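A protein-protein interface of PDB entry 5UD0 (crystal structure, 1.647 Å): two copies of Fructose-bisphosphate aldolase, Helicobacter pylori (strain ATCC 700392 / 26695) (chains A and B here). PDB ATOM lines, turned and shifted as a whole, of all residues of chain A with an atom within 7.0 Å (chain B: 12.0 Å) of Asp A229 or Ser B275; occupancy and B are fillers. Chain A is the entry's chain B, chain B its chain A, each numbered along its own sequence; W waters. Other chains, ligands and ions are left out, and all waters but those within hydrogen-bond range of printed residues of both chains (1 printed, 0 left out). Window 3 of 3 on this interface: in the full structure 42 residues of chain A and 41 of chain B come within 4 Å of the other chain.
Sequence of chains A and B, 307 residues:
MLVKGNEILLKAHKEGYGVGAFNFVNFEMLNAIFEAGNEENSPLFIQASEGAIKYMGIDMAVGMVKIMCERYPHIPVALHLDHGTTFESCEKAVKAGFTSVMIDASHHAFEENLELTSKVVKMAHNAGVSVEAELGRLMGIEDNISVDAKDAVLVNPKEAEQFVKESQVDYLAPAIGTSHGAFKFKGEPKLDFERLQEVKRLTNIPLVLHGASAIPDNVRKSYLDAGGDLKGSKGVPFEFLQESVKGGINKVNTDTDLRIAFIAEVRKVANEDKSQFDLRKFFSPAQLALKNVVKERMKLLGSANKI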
ATOM      1  N   PHE A 183       9.086 -33.549 -14.040  1.00  0.00           N
ATOM      2  CA  PHE A 183       8.194 -33.799 -15.175  1.00  0.00           C
ATOM      3  C   PHE A 183       7.127 -34.792 -14.734  1.00  0.00           C
ATOM      4  O   PHE A 183       7.106 -35.955 -15.157  1.00  0.00           O
ATOM      5  CB  PHE A 183       8.999 -34.310 -16.375  1.00  0.00           C
ATOM      6  CG  PHE A 183      10.179 -33.448 -16.689  1.00  0.00           C
ATOM      7  CD1 PHE A 183      10.028 -32.271 -17.409  1.00  0.00           C
ATOM      8  CD2 PHE A 183      11.428 -33.763 -16.186  1.00  0.00           C
ATOM      9  CE1 PHE A 183      11.119 -31.452 -17.665  1.00  0.00           C
ATOM     10  CE2 PHE A 183      12.517 -32.951 -16.439  1.00  0.00           C
ATOM     11  CZ  PHE A 183      12.362 -31.794 -17.179  1.00  0.00           C
ATOM     12  N   TYR A 223      15.365 -20.066 -12.275  1.00  0.00           N
ATOM     13  CA  TYR A 223      16.179 -21.026 -13.009  1.00  0.00           C
ATOM     14  C   TYR A 223      16.317 -20.625 -14.475  1.00  0.00           C
ATOM     15  O   TYR A 223      17.416 -20.653 -15.039  1.00  0.00           O
ATOM     16  CB  TYR A 223      15.587 -22.423 -12.900  1.00  0.00           C
ATOM     17  CG  TYR A 223      16.549 -23.488 -13.372  1.00  0.00           C
ATOM     18  CD1 TYR A 223      16.373 -24.146 -14.581  1.00  0.00           C
ATOM     19  CD2 TYR A 223      17.646 -23.845 -12.593  1.00  0.00           C
ATOM     20  CE1 TYR A 223      17.274 -25.132 -15.004  1.00  0.00           C
ATOM     21  CE2 TYR A 223      18.536 -24.816 -13.008  1.00  0.00           C
ATOM     22  CZ  TYR A 223      18.346 -25.462 -14.202  1.00  0.00           C
ATOM     23  OH  TYR A 223      19.252 -26.417 -14.603  1.00  0.00           O
ATOM     24  N   LEU A 224      15.200 -20.272 -15.122  1.00  0.00           N
ATOM     25  CA  LEU A 224      15.249 -19.936 -16.545  1.00  0.00           C
ATOM     26  C   LEU A 224      16.010 -18.638 -16.794  1.00  0.00           C
ATOM     27  O   LEU A 224      16.738 -18.523 -17.789  1.00  0.00           O
ATOM     28  CB  LEU A 224      13.830 -19.840 -17.109  1.00  0.00           C
ATOM     29  CG  LEU A 224      13.041 -21.150 -17.091  1.00  0.00           C
ATOM     30  CD1 LEU A 224      11.601 -20.874 -17.515  1.00  0.00           C
ATOM     31  CD2 LEU A 224      13.675 -22.210 -17.977  1.00  0.00           C
ATOM     32  N   GLY A 227      19.601 -18.942 -17.359  1.00  0.00           N
ATOM     33  CA  GLY A 227      19.972 -19.708 -18.530  1.00  0.00           C
ATOM     34  C   GLY A 227      19.611 -21.171 -18.493  1.00  0.00           C
ATOM     35  O   GLY A 227      20.013 -21.913 -19.400  1.00  0.00           O
ATOM     36  N   GLY A 228      18.844 -21.616 -17.496  1.00  0.00           N
ATOM     37  CA  GLY A 228      18.514 -23.023 -17.399  1.00  0.00           C
ATOM     38  C   GLY A 228      17.391 -23.434 -18.337  1.00  0.00           C
ATOM     39  O   GLY A 228      16.664 -22.609 -18.880  1.00  0.00           O
ATOM     40  N   ASP A 229      17.252 -24.747 -18.523  1.00  0.00           N
ATOM     41  CA  ASP A 229      16.203 -25.320 -19.366  1.00  0.00           C
ATOM     42  C   ASP A 229      15.302 -26.198 -18.503  1.00  0.00           C
ATOM     43  O   ASP A 229      15.774 -27.166 -17.896  1.00  0.00           O
ATOM     44  CB  ASP A 229      16.805 -26.115 -20.523  1.00  0.00           C
ATOM     45  CG  ASP A 229      15.753 -26.842 -21.345  1.00  0.00           C
ATOM     46  OD1 ASP A 229      16.034 -27.964 -21.826  1.00  0.00           O
ATOM     47  OD2 ASP A 229      14.637 -26.295 -21.494  1.00  0.00           O
ATOM     48  N   LEU A 230      14.013 -25.844 -18.437  1.00  0.00           N
ATOM     49  CA  LEU A 230      12.978 -26.614 -17.738  1.00  0.00           C
ATOM     50  C   LEU A 230      11.777 -26.845 -18.655  1.00  0.00           C
ATOM     51  O   LEU A 230      10.620 -26.640 -18.274  1.00  0.00           O
ATOM     52  CB  LEU A 230      12.503 -25.921 -16.465  1.00  0.00           C
ATOM     53  CG  LEU A 230      13.458 -25.892 -15.277  1.00  0.00           C
ATOM     54  CD1 LEU A 230      12.883 -25.005 -14.164  1.00  0.00           C
ATOM     55  CD2 LEU A 230      13.711 -27.297 -14.762  1.00  0.00           C
ATOM     56  N   LYS A 231      12.049 -27.325 -19.866  1.00  0.00           N
ATOM     57  CA  LYS A 231      11.001 -27.524 -20.864  1.00  0.00           C
ATOM     58  C   LYS A 231      10.065 -28.646 -20.418  1.00  0.00           C
ATOM     59  O   LYS A 231      10.503 -29.777 -20.175  1.00  0.00           O
ATOM     60  CB  LYS A 231      11.622 -27.839 -22.229  1.00  0.00           C
ATOM     61  CG  LYS A 231      10.809 -27.345 -23.437  1.00  0.00           C
ATOM     62  CD  LYS A 231      11.595 -27.460 -24.748  1.00  0.00           C
ATOM     63  CE  LYS A 231      11.390 -28.814 -25.451  1.00  0.00           C
ATOM     64  NZ  LYS A 231      10.223 -28.861 -26.407  1.00  0.00           N
ATOM     65  N   GLY A 232       8.776 -28.323 -20.293  1.00  0.00           N
ATOM     66  CA  GLY A 232       7.760 -29.301 -19.960  1.00  0.00           C
ATOM     67  C   GLY A 232       7.624 -29.622 -18.489  1.00  0.00           C
ATOM     68  O   GLY A 232       6.826 -30.500 -18.137  1.00  0.00           O
ATOM     69  N   SER A 233       8.368 -28.946 -17.619  1.00  0.00           N
ATOM     70  CA  SER A 233       8.340 -29.282 -16.200  1.00  0.00           C
ATOM     71  C   SER A 233       6.980 -28.968 -15.580  1.00  0.00           C
ATOM     72  O   SER A 233       6.351 -27.954 -15.890  1.00  0.00           O
ATOM     73  CB  SER A 233       9.433 -28.516 -15.459  1.00  0.00           C
ATOM     74  OG  SER A 233       9.269 -27.118 -15.623  1.00  0.00           O
ATOM     75  N   ARG A 267      24.119 -20.899 -11.222  1.00  0.00           N
ATOM     76  CA  ARG A 267      24.167 -20.479 -12.624  1.00  0.00           C
ATOM     77  C   ARG A 267      24.210 -18.967 -12.746  1.00  0.00           C
ATOM     78  O   ARG A 267      24.962 -18.418 -13.566  1.00  0.00           O
ATOM     79  CB  ARG A 267      22.958 -21.030 -13.386  1.00  0.00           C
ATOM     80  CG  ARG A 267      22.973 -22.552 -13.627  1.00  0.00           C
ATOM     81  CD  ARG A 267      21.688 -23.051 -14.276  1.00  0.00           C
ATOM     82  NE  ARG A 267      21.765 -24.475 -14.546  1.00  0.00           N
ATOM     83  CZ  ARG A 267      22.450 -25.017 -15.558  1.00  0.00           C
ATOM     84  NH1 ARG A 267      23.091 -24.246 -16.434  1.00  0.00           N
ATOM     85  NH2 ARG A 267      22.474 -26.335 -15.716  1.00  0.00           N
ATOM     86  N   VAL B 266      32.493 -26.551 -12.337  1.00  0.00           N
ATOM     87  CA  VAL B 266      31.123 -26.105 -12.081  1.00  0.00           C
ATOM     88  C   VAL B 266      30.599 -25.305 -13.268  1.00  0.00           C
ATOM     89  O   VAL B 266      29.506 -25.570 -13.786  1.00  0.00           O
ATOM     90  CB  VAL B 266      31.073 -25.282 -10.787  1.00  0.00           C
ATOM     91  CG1 VAL B 266      29.687 -24.696 -10.558  1.00  0.00           C
ATOM     92  CG2 VAL B 266      31.460 -26.147  -9.607  1.00  0.00           C
ATOM     93  N   ARG B 267      31.378 -24.310 -13.710  1.00  0.00           N
ATOM     94  CA  ARG B 267      31.028 -23.513 -14.883  1.00  0.00           C
ATOM     95  C   ARG B 267      30.823 -24.398 -16.108  1.00  0.00           C
ATOM     96  O   ARG B 267      29.883 -24.191 -16.893  1.00  0.00           O
ATOM     97  CB  ARG B 267      32.133 -22.471 -15.150  1.00  0.00           C
ATOM     98  CG  ARG B 267      32.169 -21.310 -14.124  1.00  0.00           C
ATOM     99  CD  ARG B 267      33.281 -20.277 -14.427  1.00  0.00           C
ATOM    100  NE  ARG B 267      33.263 -19.197 -13.446  1.00  0.00           N
ATOM    101  CZ  ARG B 267      32.477 -18.127 -13.520  1.00  0.00           C
ATOM    102  NH1 ARG B 267      31.642 -17.967 -14.538  1.00  0.00           N
ATOM    103  NH2 ARG B 267      32.509 -17.227 -12.554  1.00  0.00           N
ATOM    104  N   LYS B 268      31.678 -25.412 -16.263  1.00  0.00           N
ATOM    105  CA  LYS B 268      31.616 -26.314 -17.410  1.00  0.00           C
ATOM    106  C   LYS B 268      30.294 -27.074 -17.442  1.00  0.00           C
ATOM    107  O   LYS B 268      29.615 -27.111 -18.472  1.00  0.00           O
ATOM    108  CB  LYS B 268      32.804 -27.277 -17.362  1.00  0.00           C
ATOM    109  CG  LYS B 268      32.783 -28.408 -18.395  1.00  0.00           C
ATOM    110  CD  LYS B 268      34.095 -29.219 -18.383  1.00  0.00           C
ATOM    111  CE  LYS B 268      34.001 -30.516 -19.205  1.00  0.00           C
ATOM    112  NZ  LYS B 268      33.868 -30.264 -20.655  1.00  0.00           N
ATOM    113  N   VAL B 269      29.911 -27.693 -16.316  1.00  0.00           N
ATOM    114  CA  VAL B 269      28.636 -28.412 -16.259  1.00  0.00           C
ATOM    115  C   VAL B 269      27.477 -27.472 -16.567  1.00  0.00           C
ATOM    116  O   VAL B 269      26.547 -27.828 -17.300  1.00  0.00           O
ATOM    117  CB  VAL B 269      28.470 -29.092 -14.881  1.00  0.00           C
ATOM    118  CG1 VAL B 269      27.084 -29.702 -14.695  1.00  0.00           C
ATOM    119  CG2 VAL B 269      29.527 -30.164 -14.720  1.00  0.00           C
ATOM    120  N   ALA B 270      27.491 -26.274 -15.983  1.00  0.00           N
ATOM    121  CA  ALA B 270      26.429 -25.314 -16.268  1.00  0.00           C
ATOM    122  C   ALA B 270      26.336 -25.043 -17.761  1.00  0.00           C
ATOM    123  O   ALA B 270      25.239 -25.023 -18.328  1.00  0.00           O
ATOM    124  CB  ALA B 270      26.670 -24.006 -15.512  1.00  0.00           C
ATOM    125  N   ASN B 271      27.485 -24.858 -18.415  1.00  0.00           N
ATOM    126  CA  ASN B 271      27.493 -24.520 -19.835  1.00  0.00           C
ATOM    127  C   ASN B 271      26.938 -25.656 -20.689  1.00  0.00           C
ATOM    128  O   ASN B 271      26.168 -25.412 -21.628  1.00  0.00           O
ATOM    129  CB  ASN B 271      28.919 -24.193 -20.290  1.00  0.00           C
ATOM    130  CG  ASN B 271      29.504 -22.999 -19.585  1.00  0.00           C
ATOM    131  OD1 ASN B 271      28.784 -22.124 -19.128  1.00  0.00           O
ATOM    132  ND2 ASN B 271      30.835 -22.946 -19.509  1.00  0.00           N
ATOM    133  N   GLU B 272      27.334 -26.897 -20.392  1.00  0.00           N
ATOM    134  CA  GLU B 272      27.142 -28.025 -21.300  1.00  0.00           C
ATOM    135  C   GLU B 272      25.789 -28.721 -21.158  1.00  0.00           C
ATOM    136  O   GLU B 272      25.446 -29.533 -22.018  1.00  0.00           O
ATOM    137  CB  GLU B 272      28.259 -29.059 -21.105  1.00  0.00           C
ATOM    138  CG  GLU B 272      29.653 -28.550 -21.474  1.00  0.00           C
ATOM    139  CD  GLU B 272      30.711 -29.657 -21.514  1.00  0.00           C
ATOM    140  OE1 GLU B 272      30.470 -30.759 -20.971  1.00  0.00           O
ATOM    141  OE2 GLU B 272      31.792 -29.424 -22.103  1.00  0.00           O
ATOM    142  N   ASP B 273      25.018 -28.430 -20.111  1.00  0.00           N
ATOM    143  CA  ASP B 273      23.680 -29.007 -19.960  1.00  0.00           C
ATOM    144  C   ASP B 273      22.872 -27.998 -19.159  1.00  0.00           C
ATOM    145  O   ASP B 273      22.971 -27.962 -17.927  1.00  0.00           O
ATOM    146  CB  ASP B 273      23.706 -30.363 -19.270  1.00  0.00           C
ATOM    147  CG  ASP B 273      22.344 -31.050 -19.270  1.00  0.00           C
ATOM    148  OD1 ASP B 273      21.347 -30.398 -19.635  1.00  0.00           O
ATOM    149  OD2 ASP B 273      22.272 -32.244 -18.915  1.00  0.00           O
ATOM    150  N   LYS B 274      22.079 -27.190 -19.863  1.00  0.00           N
ATOM    151  CA  LYS B 274      21.205 -26.233 -19.207  1.00  0.00           C
ATOM    152  C   LYS B 274      20.110 -26.902 -18.386  1.00  0.00           C
ATOM    153  O   LYS B 274      19.448 -26.214 -17.604  1.00  0.00           O
ATOM    154  CB  LYS B 274      20.588 -25.310 -20.252  1.00  0.00           C
ATOM    155  CG  LYS B 274      21.614 -24.538 -21.085  1.00  0.00           C
ATOM    156  CD  LYS B 274      22.560 -23.782 -20.167  1.00  0.00           C
ATOM    157  CE  LYS B 274      23.539 -22.895 -20.914  1.00  0.00           C
ATOM    158  NZ  LYS B 274      24.410 -22.138 -19.956  1.00  0.00           N
ATOM    159  N   SER B 275      19.893 -28.208 -18.544  1.00  0.00           N
ATOM    160  CA  SER B 275      18.835 -28.897 -17.811  1.00  0.00           C
ATOM    161  C   SER B 275      19.356 -29.561 -16.544  1.00  0.00           C
ATOM    162  O   SER B 275      18.577 -30.195 -15.826  1.00  0.00           O
ATOM    163  CB  SER B 275      18.163 -29.947 -18.695  1.00  0.00           C
ATOM    164  OG  SER B 275      18.938 -31.137 -18.743  1.00  0.00           O
ATOM    165  N   GLN B 276      20.643 -29.406 -16.246  1.00  0.00           N
ATOM    166  CA  GLN B 276      21.285 -30.130 -15.156  1.00  0.00           C
ATOM    167  C   GLN B 276      21.151 -29.353 -13.851  1.00  0.00           C
ATOM    168  O   GLN B 276      21.630 -28.217 -13.739  1.00  0.00           O
ATOM    169  CB  GLN B 276      22.760 -30.380 -15.467  1.00  0.00           C
ATOM    170  CG  GLN B 276      23.469 -31.182 -14.384  1.00  0.00           C
ATOM    171  CD  GLN B 276      22.886 -32.573 -14.226  1.00  0.00           C
ATOM    172  OE1 GLN B 276      22.097 -32.849 -13.321  1.00  0.00           O
ATOM    173  NE2 GLN B 276      23.266 -33.464 -15.125  1.00  0.00           N
ATOM    174  N   PHE B 277      20.506 -29.970 -12.857  1.00  0.00           N
ATOM    175  CA  PHE B 277      20.440 -29.349 -11.538  1.00  0.00           C
ATOM    176  C   PHE B 277      20.678 -30.361 -10.419  1.00  0.00           C
ATOM    177  O   PHE B 277      20.381 -30.066  -9.251  1.00  0.00           O
ATOM    178  CB  PHE B 277      19.101 -28.614 -11.330  1.00  0.00           C
ATOM    179  CG  PHE B 277      17.885 -29.407 -11.731  1.00  0.00           C
ATOM    180  CD1 PHE B 277      17.351 -30.364 -10.890  1.00  0.00           C
ATOM    181  CD2 PHE B 277      17.265 -29.164 -12.938  1.00  0.00           C
ATOM    182  CE1 PHE B 277      16.221 -31.069 -11.251  1.00  0.00           C
ATOM    183  CE2 PHE B 277      16.148 -29.863 -13.308  1.00  0.00           C
ATOM    184  CZ  PHE B 277      15.623 -30.817 -12.478  1.00  0.00           C
ATOM    185  N   ASP B 278      21.245 -31.528 -10.733  1.00  0.00           N
ATOM    186  CA  ASP B 278      21.728 -32.438  -9.707  1.00  0.00           C
ATOM    187  C   ASP B 278      23.073 -31.906  -9.212  1.00  0.00           C
ATOM    188  O   ASP B 278      24.064 -31.867  -9.968  1.00  0.00           O
ATOM    189  CB  ASP B 278      21.830 -33.855 -10.265  1.00  0.00           C
ATOM    190  CG  ASP B 278      22.303 -34.889  -9.229  1.00  0.00           C
ATOM    191  OD1 ASP B 278      22.843 -34.529  -8.155  1.00  0.00           O
ATOM    192  OD2 ASP B 278      22.134 -36.084  -9.525  1.00  0.00           O
ATOM    193  N   LEU B 279      23.110 -31.509  -7.929  1.00  0.00           N
ATOM    194  CA  LEU B 279      24.318 -30.901  -7.364  1.00  0.00           C
ATOM    195  C   LEU B 279      25.528 -31.802  -7.529  1.00  0.00           C
ATOM    196  O   LEU B 279      26.648 -31.317  -7.740  1.00  0.00           O
ATOM    197  CB  LEU B 279      24.119 -30.588  -5.880  1.00  0.00           C
ATOM    198  CG  LEU B 279      23.455 -29.236  -5.533  1.00  0.00           C
ATOM    199  CD1 LEU B 279      21.985 -29.229  -5.918  1.00  0.00           C
ATOM    200  CD2 LEU B 279      23.639 -28.927  -4.049  1.00  0.00           C
ATOM    201  N   ARG B 280      25.339 -33.115  -7.357  1.00  0.00           N
ATOM    202  CA  ARG B 280      26.453 -34.056  -7.471  1.00  0.00           C
ATOM    203  C   ARG B 280      27.040 -34.080  -8.876  1.00  0.00           C
ATOM    204  O   ARG B 280      28.244 -34.314  -9.044  1.00  0.00           O
ATOM    205  CB  ARG B 280      25.991 -35.453  -7.047  1.00  0.00           C
ATOM    206  CG  ARG B 280      25.555 -35.539  -5.576  1.00  0.00           C
ATOM    207  CD  ARG B 280      24.639 -36.739  -5.288  1.00  0.00           C
ATOM    208  NE  ARG B 280      23.373 -36.583  -6.000  1.00  0.00           N
ATOM    209  CZ  ARG B 280      22.295 -37.343  -5.832  1.00  0.00           C
ATOM    210  NH1 ARG B 280      22.299 -38.348  -4.963  1.00  0.00           N
ATOM    211  NH2 ARG B 280      21.206 -37.093  -6.545  1.00  0.00           N
ATOM    212  N   LYS B 281      26.225 -33.833  -9.901  1.00  0.00           N
ATOM    213  CA  LYS B 281      26.761 -33.727 -11.253  1.00  0.00           C
ATOM    214  C   LYS B 281      27.657 -32.507 -11.418  1.00  0.00           C
ATOM    215  O   LYS B 281      28.547 -32.509 -12.266  1.00  0.00           O
ATOM    216  CB  LYS B 281      25.636 -33.671 -12.277  1.00  0.00           C
ATOM    217  CG  LYS B 281      24.850 -34.968 -12.383  1.00  0.00           C
ATOM    218  CD  LYS B 281      25.670 -36.080 -13.013  1.00  0.00           C
ATOM    219  CE  LYS B 281      24.901 -37.396 -13.072  1.00  0.00           C
ATOM    220  NZ  LYS B 281      25.695 -38.435 -13.770  1.00  0.00           N
ATOM    221  N   PHE B 282      27.414 -31.444 -10.657  1.00  0.00           N
ATOM    222  CA  PHE B 282      28.330 -30.311 -10.681  1.00  0.00           C
ATOM    223  C   PHE B 282      29.584 -30.577  -9.863  1.00  0.00           C
ATOM    224  O   PHE B 282      30.691 -30.237 -10.293  1.00  0.00           O
ATOM    225  CB  PHE B 282      27.644 -29.059 -10.147  1.00  0.00           C
ATOM    226  CG  PHE B 282      26.647 -28.465 -11.085  1.00  0.00           C
ATOM    227  CD1 PHE B 282      25.309 -28.844 -11.039  1.00  0.00           C
ATOM    228  CD2 PHE B 282      27.035 -27.512 -12.000  1.00  0.00           C
ATOM    229  CE1 PHE B 282      24.402 -28.305 -11.911  1.00  0.00           C
ATOM    230  CE2 PHE B 282      26.114 -26.950 -12.870  1.00  0.00           C
ATOM    231  CZ  PHE B 282      24.815 -27.352 -12.834  1.00  0.00           C
HETATM  232  O   HOH W   1      23.146 -21.377 -17.074  1.00  0.00           O
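The backbone carbonyl oxygen of Gln B276 is in hydrogen-bond range of the side-chain hydroxyl of Tyr A223.
The backbone carbonyl oxygen (O) of Ala B270 is in hydrogen-bond range of the guanidinium group (NH1) of Arg A267 (3.0 Å).
The backbone NH (N) of Asp A229 is in hydrogen-bond range of the backbone carbonyl oxygen (O) of Lys B274 (2.8 Å).
O of Gln B276 is in hydrogen-bond range of NH2 of Arg A267 (2.9 Å).
O of Asp B273 lies within hydrogen-bond range of NH2 of Arg A267 (2.8 Å).
O of Lys B274 sits at hydrogen-bond distance from OH of Tyr A223 (3.0 Å).
OH of Tyr A223 sits at hydrogen-bond distance from NE of Arg A267 (3.2 Å).
O of Ala B270 sits at hydrogen-bond distance from NZ of Lys B274 (3.4 Å).
The side-chain amide oxygen (OE1) of Gln B276 sits at hydrogen-bond distance from the backbone NH (N) of Asp B278 (3.0 Å).
The side-chain carboxylate (OD2) of Asp A229 lies within hydrogen-bond range of the backbone NH (N) of Lys A231, 3.2 Å away.
OG of Ser B275 is in hydrogen-bond range of OD1 of Asp B273 (2.7 Å).
OG of Ser A233 sits at hydrogen-bond distance from O of Leu A230, 3.0 Å away.
Among the printed residues, pairs that only touch across the chains: Gly A227 with Lys B274, Gly A228 with Lys B274, Asp A229 with Ser B275, Arg A267 with Lys B274, Tyr A223 with Ser B275, Tyr A223 with Phe B277, Leu A230 with Phe B277 and Arg A267 with Phe B282.
Asp A229 touches just these residues of chain B: Lys B274 (2.8 Å) and Ser B275 (3.5 Å).
Ser B275 touches just these residues of chain A: Tyr A223 (3.7 Å) and Asp A229 (3.5 Å).
Gly A227 touches just one residue of chain B: Lys B274 (3.3 Å).
Gly A228 touches one residue of chain B.
No residue of chain B comes within 4 Å of Lys A231.
Of the printed residues of chain A, Gln B276 touches Tyr A223 and Arg A267.
Of the printed residues of chain A, Phe B277 touches Tyr A223 and Leu A230.
Leu B279 touches none of the printed residues of chain A.
Asp B278 touches none of the printed residues of chain A.
Of the 17 printed residues of chain B, 7 touch a printed residue of chain A.
Along chain B the printed residues that touch a printed residue of chain A span positions 270 to 282.
Among the printed residues, 14 pairs touch across the chains.
Position printed for both chains: 267.
Of the 14 pairs that touch across the chains among the printed residues, none has its exchanged pair printed and touching as well.
Water W1 bridges NH1 of Arg A267 (2.9 Å) and NZ of Lys B274 (3.2 Å).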
